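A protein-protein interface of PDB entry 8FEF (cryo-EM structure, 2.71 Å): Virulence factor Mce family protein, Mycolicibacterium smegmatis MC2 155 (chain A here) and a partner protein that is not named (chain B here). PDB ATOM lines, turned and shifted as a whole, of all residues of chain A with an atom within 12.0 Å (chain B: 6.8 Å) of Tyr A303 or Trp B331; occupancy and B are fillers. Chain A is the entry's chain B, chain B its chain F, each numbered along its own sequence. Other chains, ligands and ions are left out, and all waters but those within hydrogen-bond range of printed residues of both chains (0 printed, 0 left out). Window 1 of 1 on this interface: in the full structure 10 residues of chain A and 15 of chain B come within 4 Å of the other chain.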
ATOM      1  N   LYS A 294      26.782  25.684  27.524  1.00  0.00           N
ATOM      2  CA  LYS A 294      26.321  24.748  26.502  1.00  0.00           C
ATOM      3  C   LYS A 294      25.001  25.201  25.890  1.00  0.00           C
ATOM      4  O   LYS A 294      24.825  25.158  24.661  1.00  0.00           O
ATOM      5  CB  LYS A 294      26.179  23.347  27.098  1.00  0.00           C
ATOM      6  CG  LYS A 294      27.433  22.499  26.992  1.00  0.00           C
ATOM      7  CD  LYS A 294      27.265  21.162  27.689  1.00  0.00           C
ATOM      8  CE  LYS A 294      27.522  21.290  29.176  1.00  0.00           C
ATOM      9  NZ  LYS A 294      28.909  21.754  29.450  1.00  0.00           N
ATOM     10  N   ILE A 295      24.032  25.578  26.709  1.00  0.00           N
ATOM     11  CA  ILE A 295      22.733  25.983  26.173  1.00  0.00           C
ATOM     12  C   ILE A 295      22.866  27.149  25.210  1.00  0.00           C
ATOM     13  O   ILE A 295      22.417  27.106  24.052  1.00  0.00           O
ATOM     14  CB  ILE A 295      21.763  26.373  27.298  1.00  0.00           C
ATOM     15  CG1 ILE A 295      21.294  25.139  28.052  1.00  0.00           C
ATOM     16  CG2 ILE A 295      20.548  27.063  26.734  1.00  0.00           C
ATOM     17  CD1 ILE A 295      20.238  25.433  29.087  1.00  0.00           C
ATOM     18  N   ILE A 296      23.564  28.169  25.680  1.00  0.00           N
ATOM     19  CA  ILE A 296      23.751  29.380  24.920  1.00  0.00           C
ATOM     20  C   ILE A 296      24.475  29.134  23.611  1.00  0.00           C
ATOM     21  O   ILE A 296      24.127  29.734  22.600  1.00  0.00           O
ATOM     22  CB  ILE A 296      24.437  30.472  25.759  1.00  0.00           C
ATOM     23  CG1 ILE A 296      24.689  31.712  24.934  1.00  0.00           C
ATOM     24  CG2 ILE A 296      25.752  30.000  26.318  1.00  0.00           C
ATOM     25  CD1 ILE A 296      25.639  32.665  25.615  1.00  0.00           C
ATOM     26  N   GLY A 297      25.462  28.254  23.601  1.00  0.00           N
ATOM     27  CA  GLY A 297      26.183  28.015  22.374  1.00  0.00           C
ATOM     28  C   GLY A 297      25.267  27.474  21.318  1.00  0.00           C
ATOM     29  O   GLY A 297      25.218  27.998  20.228  1.00  0.00           O
ATOM     30  N   ARG A 298      24.449  26.500  21.666  1.00  0.00           N
ATOM     31  CA  ARG A 298      23.533  25.945  20.692  1.00  0.00           C
ATOM     32  C   ARG A 298      22.499  26.970  20.251  1.00  0.00           C
ATOM     33  O   ARG A 298      22.043  26.947  19.118  1.00  0.00           O
ATOM     34  CB  ARG A 298      22.910  24.633  21.139  1.00  0.00           C
ATOM     35  CG  ARG A 298      22.967  23.606  20.024  1.00  0.00           C
ATOM     36  CD  ARG A 298      21.850  22.593  20.096  1.00  0.00           C
ATOM     37  NE  ARG A 298      21.579  22.038  18.779  1.00  0.00           N
ATOM     38  CZ  ARG A 298      22.515  21.558  17.977  1.00  0.00           C
ATOM     39  NH1 ARG A 298      23.776  21.593  18.356  1.00  0.00           N
ATOM     40  NH2 ARG A 298      22.194  21.055  16.795  1.00  0.00           N
ATOM     41  N   ALA A 299      22.048  27.812  21.167  1.00  0.00           N
ATOM     42  CA  ALA A 299      21.103  28.858  20.781  1.00  0.00           C
ATOM     43  C   ALA A 299      21.672  29.884  19.804  1.00  0.00           C
ATOM     44  O   ALA A 299      20.983  30.321  18.901  1.00  0.00           O
ATOM     45  CB  ALA A 299      20.562  29.569  22.003  1.00  0.00           C
ATOM     46  N   GLY A 300      22.932  30.265  19.979  1.00  0.00           N
ATOM     47  CA  GLY A 300      23.534  31.316  19.161  1.00  0.00           C
ATOM     48  C   GLY A 300      23.902  31.333  17.677  1.00  0.00           C
ATOM     49  O   GLY A 300      23.406  32.161  16.940  1.00  0.00           O
ATOM     50  N   GLY A 301      24.785  30.449  17.243  1.00  0.00           N
ATOM     51  CA  GLY A 301      25.312  30.408  15.887  1.00  0.00           C
ATOM     52  C   GLY A 301      25.447  29.067  15.193  1.00  0.00           C
ATOM     53  O   GLY A 301      26.238  28.945  14.255  1.00  0.00           O
ATOM     54  N   ILE A 302      24.709  28.049  15.632  1.00  0.00           N
ATOM     55  CA  ILE A 302      24.814  26.741  14.989  1.00  0.00           C
ATOM     56  C   ILE A 302      24.188  26.753  13.596  1.00  0.00           C
ATOM     57  O   ILE A 302      24.735  26.168  12.654  1.00  0.00           O
ATOM     58  CB  ILE A 302      24.196  25.648  15.878  1.00  0.00           C
ATOM     59  CG1 ILE A 302      22.780  26.025  16.311  1.00  0.00           C
ATOM     60  CG2 ILE A 302      25.076  25.402  17.093  1.00  0.00           C
ATOM     61  CD1 ILE A 302      22.052  24.911  17.006  1.00  0.00           C
ATOM     62  N   TYR A 303      23.040  27.412  13.436  1.00  0.00           N
ATOM     63  CA  TYR A 303      22.293  27.322  12.185  1.00  0.00           C
ATOM     64  C   TYR A 303      22.909  28.150  11.066  1.00  0.00           C
ATOM     65  O   TYR A 303      22.732  27.818   9.890  1.00  0.00           O
ATOM     66  CB  TYR A 303      20.843  27.752  12.411  1.00  0.00           C
ATOM     67  CG  TYR A 303      20.050  26.809  13.287  1.00  0.00           C
ATOM     68  CD1 TYR A 303      20.478  25.508  13.506  1.00  0.00           C
ATOM     69  CD2 TYR A 303      18.870  27.217  13.887  1.00  0.00           C
ATOM     70  CE1 TYR A 303      19.755  24.645  14.297  1.00  0.00           C
ATOM     71  CE2 TYR A 303      18.141  26.360  14.682  1.00  0.00           C
ATOM     72  CZ  TYR A 303      18.590  25.074  14.883  1.00  0.00           C
ATOM     73  OH  TYR A 303      17.870  24.211  15.674  1.00  0.00           O
ATOM     74  N   GLY A 304      23.618  29.220  11.400  1.00  0.00           N
ATOM     75  CA  GLY A 304      24.162  30.090  10.377  1.00  0.00           C
ATOM     76  C   GLY A 304      24.822  31.292  11.012  1.00  0.00           C
ATOM     77  O   GLY A 304      25.200  31.261  12.183  1.00  0.00           O
ATOM     78  N   ASP A 305      24.949  32.351  10.224  1.00  0.00           N
ATOM     79  CA  ASP A 305      25.547  33.590  10.701  1.00  0.00           C
ATOM     80  C   ASP A 305      24.586  34.425  11.543  1.00  0.00           C
ATOM     81  O   ASP A 305      24.854  35.604  11.783  1.00  0.00           O
ATOM     82  CB  ASP A 305      26.045  34.412   9.510  1.00  0.00           C
ATOM     83  CG  ASP A 305      27.138  35.375   9.892  1.00  0.00           C
ATOM     84  OD1 ASP A 305      27.706  35.190  10.982  1.00  0.00           O
ATOM     85  OD2 ASP A 305      27.420  36.314   9.118  1.00  0.00           O
ATOM     86  N   PHE A 306      23.475  33.847  11.987  1.00  0.00           N
ATOM     87  CA  PHE A 306      22.423  34.577  12.673  1.00  0.00           C
ATOM     88  C   PHE A 306      22.121  33.964  14.034  1.00  0.00           C
ATOM     89  O   PHE A 306      22.239  32.751  14.227  1.00  0.00           O
ATOM     90  CB  PHE A 306      21.153  34.601  11.820  1.00  0.00           C
ATOM     91  CG  PHE A 306      20.795  33.269  11.230  1.00  0.00           C
ATOM     92  CD1 PHE A 306      20.111  32.324  11.971  1.00  0.00           C
ATOM     93  CD2 PHE A 306      21.137  32.965   9.926  1.00  0.00           C
ATOM     94  CE1 PHE A 306      19.781  31.102  11.427  1.00  0.00           C
ATOM     95  CE2 PHE A 306      20.810  31.745   9.375  1.00  0.00           C
ATOM     96  CZ  PHE A 306      20.128  30.812  10.126  1.00  0.00           C
ATOM     97  N   PHE A 307      21.733  34.820  14.978  1.00  0.00           N
ATOM     98  CA  PHE A 307      21.201  34.354  16.248  1.00  0.00           C
ATOM     99  C   PHE A 307      19.840  33.697  16.035  1.00  0.00           C
ATOM    100  O   PHE A 307      19.215  33.819  14.979  1.00  0.00           O
ATOM    101  CB  PHE A 307      21.070  35.507  17.241  1.00  0.00           C
ATOM    102  CG  PHE A 307      22.333  35.817  17.983  1.00  0.00           C
ATOM    103  CD1 PHE A 307      22.646  35.143  19.149  1.00  0.00           C
ATOM    104  CD2 PHE A 307      23.200  36.792  17.528  1.00  0.00           C
ATOM    105  CE1 PHE A 307      23.804  35.428  19.840  1.00  0.00           C
ATOM    106  CE2 PHE A 307      24.358  37.080  18.217  1.00  0.00           C
ATOM    107  CZ  PHE A 307      24.661  36.397  19.373  1.00  0.00           C
ATOM    108  N   ASN A 308      19.372  32.994  17.059  1.00  0.00           N
ATOM    109  CA  ASN A 308      18.048  32.384  17.050  1.00  0.00           C
ATOM    110  C   ASN A 308      17.195  33.072  18.106  1.00  0.00           C
ATOM    111  O   ASN A 308      17.437  32.914  19.307  1.00  0.00           O
ATOM    112  CB  ASN A 308      18.124  30.882  17.305  1.00  0.00           C
ATOM    113  CG  ASN A 308      18.627  30.116  16.109  1.00  0.00           C
ATOM    114  OD1 ASN A 308      17.889  29.891  15.152  1.00  0.00           O
ATOM    115  ND2 ASN A 308      19.886  29.701  16.155  1.00  0.00           N
ATOM    116  N   PHE A 309      16.203  33.834  17.658  1.00  0.00           N
ATOM    117  CA  PHE A 309      15.251  34.494  18.538  1.00  0.00           C
ATOM    118  C   PHE A 309      13.876  33.872  18.345  1.00  0.00           C
ATOM    119  O   PHE A 309      13.501  33.507  17.226  1.00  0.00           O
ATOM    120  CB  PHE A 309      15.186  35.997  18.263  1.00  0.00           C
ATOM    121  CG  PHE A 309      16.277  36.789  18.926  1.00  0.00           C
ATOM    122  CD1 PHE A 309      17.368  36.160  19.494  1.00  0.00           C
ATOM    123  CD2 PHE A 309      16.200  38.169  18.990  1.00  0.00           C
ATOM    124  CE1 PHE A 309      18.367  36.893  20.104  1.00  0.00           C
ATOM    125  CE2 PHE A 309      17.195  38.905  19.600  1.00  0.00           C
ATOM    126  CZ  PHE A 309      18.279  38.266  20.157  1.00  0.00           C
ATOM    127  N   TYR A 310      13.131  33.742  19.440  1.00  0.00           N
ATOM    128  CA  TYR A 310      11.773  33.214  19.407  1.00  0.00           C
ATOM    129  C   TYR A 310      10.862  34.212  20.102  1.00  0.00           C
ATOM    130  O   TYR A 310      11.085  34.548  21.268  1.00  0.00           O
ATOM    131  CB  TYR A 310      11.695  31.844  20.084  1.00  0.00           C
ATOM    132  CG  TYR A 310      10.439  31.068  19.771  1.00  0.00           C
ATOM    133  CD1 TYR A 310       9.270  31.278  20.487  1.00  0.00           C
ATOM    134  CD2 TYR A 310      10.424  30.117  18.763  1.00  0.00           C
ATOM    135  CE1 TYR A 310       8.120  30.569  20.203  1.00  0.00           C
ATOM    136  CE2 TYR A 310       9.280  29.402  18.473  1.00  0.00           C
ATOM    137  CZ  TYR A 310       8.131  29.631  19.196  1.00  0.00           C
ATOM    138  OH  TYR A 310       6.989  28.922  18.910  1.00  0.00           O
ATOM    139  N   ARG A 339       6.970  25.935  24.660  1.00  0.00           N
ATOM    140  CA  ARG A 339       8.362  26.148  25.028  1.00  0.00           C
ATOM    141  C   ARG A 339       8.531  27.299  26.008  1.00  0.00           C
ATOM    142  O   ARG A 339       9.549  27.356  26.703  1.00  0.00           O
ATOM    143  CB  ARG A 339       9.208  26.402  23.781  1.00  0.00           C
ATOM    144  CG  ARG A 339       8.748  27.585  22.963  1.00  0.00           C
ATOM    145  CD  ARG A 339       9.742  27.935  21.874  1.00  0.00           C
ATOM    146  NE  ARG A 339      10.971  28.519  22.396  1.00  0.00           N
ATOM    147  CZ  ARG A 339      12.151  27.918  22.376  1.00  0.00           C
ATOM    148  NH1 ARG A 339      12.300  26.706  21.871  1.00  0.00           N
ATOM    149  NH2 ARG A 339      13.212  28.556  22.860  1.00  0.00           N
ATOM    150  N   CYS B 321      25.279  33.919   5.762  1.00  0.00           N
ATOM    151  CA  CYS B 321      26.042  32.832   5.163  1.00  0.00           C
ATOM    152  C   CYS B 321      25.740  31.536   5.900  1.00  0.00           C
ATOM    153  O   CYS B 321      25.891  31.461   7.123  1.00  0.00           O
ATOM    154  CB  CYS B 321      27.548  33.106   5.164  1.00  0.00           C
ATOM    155  SG  CYS B 321      28.259  33.931   6.601  1.00  0.00           S
ATOM    156  N   LEU B 322      25.308  30.527   5.150  1.00  0.00           N
ATOM    157  CA  LEU B 322      25.053  29.196   5.676  1.00  0.00           C
ATOM    158  C   LEU B 322      26.191  28.233   5.368  1.00  0.00           C
ATOM    159  O   LEU B 322      26.053  27.029   5.602  1.00  0.00           O
ATOM    160  CB  LEU B 322      23.735  28.656   5.116  1.00  0.00           C
ATOM    161  CG  LEU B 322      22.550  29.629   5.091  1.00  0.00           C
ATOM    162  CD1 LEU B 322      21.319  28.966   4.501  1.00  0.00           C
ATOM    163  CD2 LEU B 322      22.249  30.161   6.480  1.00  0.00           C
ATOM    164  N   PHE B 325      28.320  26.139   8.339  1.00  0.00           N
ATOM    165  CA  PHE B 325      27.413  25.986   9.462  1.00  0.00           C
ATOM    166  C   PHE B 325      26.581  24.724   9.270  1.00  0.00           C
ATOM    167  O   PHE B 325      26.784  23.953   8.328  1.00  0.00           O
ATOM    168  CB  PHE B 325      26.518  27.213   9.608  1.00  0.00           C
ATOM    169  CG  PHE B 325      27.243  28.448  10.050  1.00  0.00           C
ATOM    170  CD1 PHE B 325      27.672  28.582  11.357  1.00  0.00           C
ATOM    171  CD2 PHE B 325      27.477  29.482   9.166  1.00  0.00           C
ATOM    172  CE1 PHE B 325      28.329  29.720  11.769  1.00  0.00           C
ATOM    173  CE2 PHE B 325      28.134  30.623   9.574  1.00  0.00           C
ATOM    174  CZ  PHE B 325      28.561  30.741  10.876  1.00  0.00           C
ATOM    175  N   LEU B 326      25.641  24.515  10.182  1.00  0.00           N
ATOM    176  CA  LEU B 326      24.831  23.309  10.156  1.00  0.00           C
ATOM    177  C   LEU B 326      23.933  23.300   8.920  1.00  0.00           C
ATOM    178  O   LEU B 326      23.429  24.349   8.511  1.00  0.00           O
ATOM    179  CB  LEU B 326      23.983  23.222  11.425  1.00  0.00           C
ATOM    180  CG  LEU B 326      23.606  21.842  11.957  1.00  0.00           C
ATOM    181  CD1 LEU B 326      24.852  21.037  12.274  1.00  0.00           C
ATOM    182  CD2 LEU B 326      22.728  21.981  13.188  1.00  0.00           C
ATOM    183  N   PRO B 327      23.727  22.142   8.298  1.00  0.00           N
ATOM    184  CA  PRO B 327      22.841  22.076   7.130  1.00  0.00           C
ATOM    185  C   PRO B 327      21.397  22.368   7.506  1.00  0.00           C
ATOM    186  O   PRO B 327      20.996  22.286   8.668  1.00  0.00           O
ATOM    187  CB  PRO B 327      23.003  20.634   6.638  1.00  0.00           C
ATOM    188  CG  PRO B 327      24.303  20.182   7.200  1.00  0.00           C
ATOM    189  CD  PRO B 327      24.431  20.870   8.521  1.00  0.00           C
ATOM    190  N   ALA B 328      20.614  22.728   6.487  1.00  0.00           N
ATOM    191  CA  ALA B 328      19.208  23.050   6.708  1.00  0.00           C
ATOM    192  C   ALA B 328      18.436  21.843   7.226  1.00  0.00           C
ATOM    193  O   ALA B 328      17.590  21.976   8.117  1.00  0.00           O
ATOM    194  CB  ALA B 328      18.579  23.572   5.418  1.00  0.00           C
ATOM    195  N   SER B 329      18.713  20.658   6.678  1.00  0.00           N
ATOM    196  CA  SER B 329      18.002  19.454   7.096  1.00  0.00           C
ATOM    197  C   SER B 329      18.329  19.045   8.525  1.00  0.00           C
ATOM    198  O   SER B 329      17.603  18.227   9.101  1.00  0.00           O
ATOM    199  CB  SER B 329      18.317  18.300   6.145  1.00  0.00           C
ATOM    200  OG  SER B 329      17.646  17.117   6.543  1.00  0.00           O
ATOM    201  N   GLN B 330      19.397  19.582   9.109  1.00  0.00           N
ATOM    202  CA  GLN B 330      19.776  19.258  10.477  1.00  0.00           C
ATOM    203  C   GLN B 330      19.224  20.244  11.497  1.00  0.00           C
ATOM    204  O   GLN B 330      19.518  20.106  12.689  1.00  0.00           O
ATOM    205  CB  GLN B 330      21.302  19.189  10.601  1.00  0.00           C
ATOM    206  CG  GLN B 330      21.959  18.200   9.649  1.00  0.00           C
ATOM    207  CD  GLN B 330      21.423  16.791   9.802  1.00  0.00           C
ATOM    208  OE1 GLN B 330      21.788  16.072  10.732  1.00  0.00           O
ATOM    209  NE2 GLN B 330      20.553  16.386   8.883  1.00  0.00           N
ATOM    210  N   TRP B 331      18.445  21.232  11.063  1.00  0.00           N
ATOM    211  CA  TRP B 331      17.822  22.163  11.991  1.00  0.00           C
ATOM    212  C   TRP B 331      16.782  21.445  12.845  1.00  0.00           C
ATOM    213  O   TRP B 331      16.152  20.476  12.412  1.00  0.00           O
ATOM    214  CB  TRP B 331      17.166  23.320  11.237  1.00  0.00           C
ATOM    215  CG  TRP B 331      18.138  24.295  10.651  1.00  0.00           C
ATOM    216  CD1 TRP B 331      19.495  24.184  10.622  1.00  0.00           C
ATOM    217  CD2 TRP B 331      17.824  25.534  10.005  1.00  0.00           C
ATOM    218  NE1 TRP B 331      20.048  25.276  10.000  1.00  0.00           N
ATOM    219  CE2 TRP B 331      19.042  26.119   9.611  1.00  0.00           C
ATOM    220  CE3 TRP B 331      16.631  26.204   9.722  1.00  0.00           C
ATOM    221  CZ2 TRP B 331      19.102  27.342   8.949  1.00  0.00           C
ATOM    222  CZ3 TRP B 331      16.692  27.417   9.065  1.00  0.00           C
ATOM    223  CH2 TRP B 331      17.918  27.974   8.686  1.00  0.00           C
ATOM    224  N   ARG B 332      16.609  21.929  14.069  1.00  0.00           N
ATOM    225  CA  ARG B 332      15.691  21.324  15.023  1.00  0.00           C
ATOM    226  C   ARG B 332      14.421  22.153  15.132  1.00  0.00           C
ATOM    227  O   ARG B 332      14.462  23.385  15.071  1.00  0.00           O
ATOM    228  CB  ARG B 332      16.352  21.182  16.395  1.00  0.00           C
ATOM    229  CG  ARG B 332      17.862  21.031  16.326  1.00  0.00           C
ATOM    230  CD  ARG B 332      18.429  20.278  17.518  1.00  0.00           C
ATOM    231  NE  ARG B 332      18.114  20.913  18.791  1.00  0.00           N
ATOM    232  CZ  ARG B 332      17.289  20.407  19.696  1.00  0.00           C
ATOM    233  NH1 ARG B 332      16.687  19.245  19.508  1.00  0.00           N
ATOM    234  NH2 ARG B 332      17.066  21.082  20.818  1.00  0.00           N
ATOM    235  N   SER B 333      13.293  21.464  15.275  1.00  0.00           N
ATOM    236  CA  SER B 333      12.010  22.138  15.392  1.00  0.00           C
ATOM    237  C   SER B 333      11.981  22.987  16.660  1.00  0.00           C
ATOM    238  O   SER B 333      12.548  22.589  17.684  1.00  0.00           O
ATOM    239  CB  SER B 333      10.875  21.113  15.412  1.00  0.00           C
ATOM    240  OG  SER B 333       9.607  21.742  15.430  1.00  0.00           O
ATOM    241  N   PRO B 334      11.352  24.165  16.627  1.00  0.00           N
ATOM    242  CA  PRO B 334      11.364  25.037  17.814  1.00  0.00           C
ATOM    243  C   PRO B 334      10.653  24.450  19.021  1.00  0.00           C
ATOM    244  O   PRO B 334      10.878  24.925  20.140  1.00  0.00           O
ATOM    245  CB  PRO B 334      10.670  26.314  17.320  1.00  0.00           C
ATOM    246  CG  PRO B 334       9.858  25.877  16.145  1.00  0.00           C
ATOM    247  CD  PRO B 334      10.640  24.780  15.495  1.00  0.00           C
ATOM    248  N   LEU B 346      32.336  25.363  13.439  1.00  0.00           N
ATOM    249  CA  LEU B 346      31.297  25.938  12.594  1.00  0.00           C
ATOM    250  C   LEU B 346      31.488  27.447  12.525  1.00  0.00           C
ATOM    251  O   LEU B 346      31.362  28.136  13.543  1.00  0.00           O
ATOM    252  CB  LEU B 346      29.904  25.606  13.128  1.00  0.00           C
ATOM    253  CG  LEU B 346      29.440  24.152  13.079  1.00  0.00           C
ATOM    254  CD1 LEU B 346      27.966  24.066  13.420  1.00  0.00           C
ATOM    255  CD2 LEU B 346      29.715  23.528  11.724  1.00  0.00           C
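Tyr A303 touches just these residues of chain B: Phe B325 (3.8 Å), Leu B326 (3.8 Å), Trp B331 (3.3 Å) and Arg B332 (3.1 Å).
Of the printed residues of chain B, Gly A304 touches Cys B321 (3.9 Å) and Phe B325 (3.5 Å).
Phe A307 touches none of the printed residues of chain B.
Printed residues of chain B within 4 Å of Tyr A310: Pro B334 (3.6 Å).
Of the printed residues of chain B, Arg A339 touches Pro B334.
Of chain A, only Phe A306 comes within 4 Å of Leu B322.
Printed residues of chain A within 4 Å of Phe B325: Gly A301 (3.3 Å), Ile A302 (3.7 Å), Tyr A303 (3.8 Å), Gly A304 (3.5 Å) and Asp A305 (3.7 Å).
Leu B326 touches just these residues of chain A: Arg A298 (3.8 Å), Ile A302 (3.1 Å) and Tyr A303 (3.8 Å).
Pro B327 touches none of the printed residues of chain A.
No residue of chain A comes within 4 Å of Ala B328.
No residue of chain A comes within 4 Å of Ser B329.
No residue of chain A comes within 4 Å of Gln B330.
Trp B331 touches two residues of chain A.
Arg B332 touches two residues of chain A.
Printed residues of chain A within 4 Å of Leu B346: Ile A302 (3.9 Å).
The nearest printed residue of chain B that does not touch Gly A301 is Leu B346 (5.1 Å).
Of the 18 printed residues of chain A, 9 touch a printed residue of chain B.
Printed residues of chain B that touch a printed residue of chain A: Cys B321, Leu B322, Phe B325, Leu B326, Trp B331, Arg B332, Pro B334 and Leu B346.
Among the printed residues, no Asp or Glu carboxylate lies within 4 Å of a Lys or Arg side-chain nitrogen of the other chain.
Among the printed residues, merely in contact across the chains: Gly A301 with Phe B325 (3.3 Å), Tyr A303 with Trp B331 (3.3 Å), Gly A304 with Phe B325 (3.5 Å), Tyr A310 with Pro B334 (3.6 Å), Phe A306 with Leu B322 (3.6 Å), Arg A298 with Arg B332 (3.6 Å), Ile A302 with Phe B325 (3.7 Å), Asp A305 with Phe B325 (3.7 Å), Arg A298 with Leu B326 (3.8 Å), Tyr A303 with Leu B326 (3.8 Å), Phe A306 with Trp B331 (3.8 Å), Tyr A303 with Phe B325 (3.8 Å), Ile A302 with Leu B346 (3.9 Å) and Gly A304 with Cys B321 (3.9 Å).
The backbone carbonyl oxygen of Pro B327 lies close to the indole nitrogen of Trp B331 (3.4 Å).
The side-chain hydroxyl of Tyr A303 sits at hydrogen-bond distance from the backbone NH of Arg B332 (3.1 Å).
The guanidinium group (NH1) of Arg A339 is in hydrogen-bond range of the backbone carbonyl oxygen (O) of Pro B334 (2.9 Å).
N of Asp A305 is in hydrogen-bond range of O of Cys B321, at 3.4 Å.
The backbone NH (N) of Leu B326 lies within hydrogen-bond range of the backbone carbonyl oxygen (O) of Ile A302.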
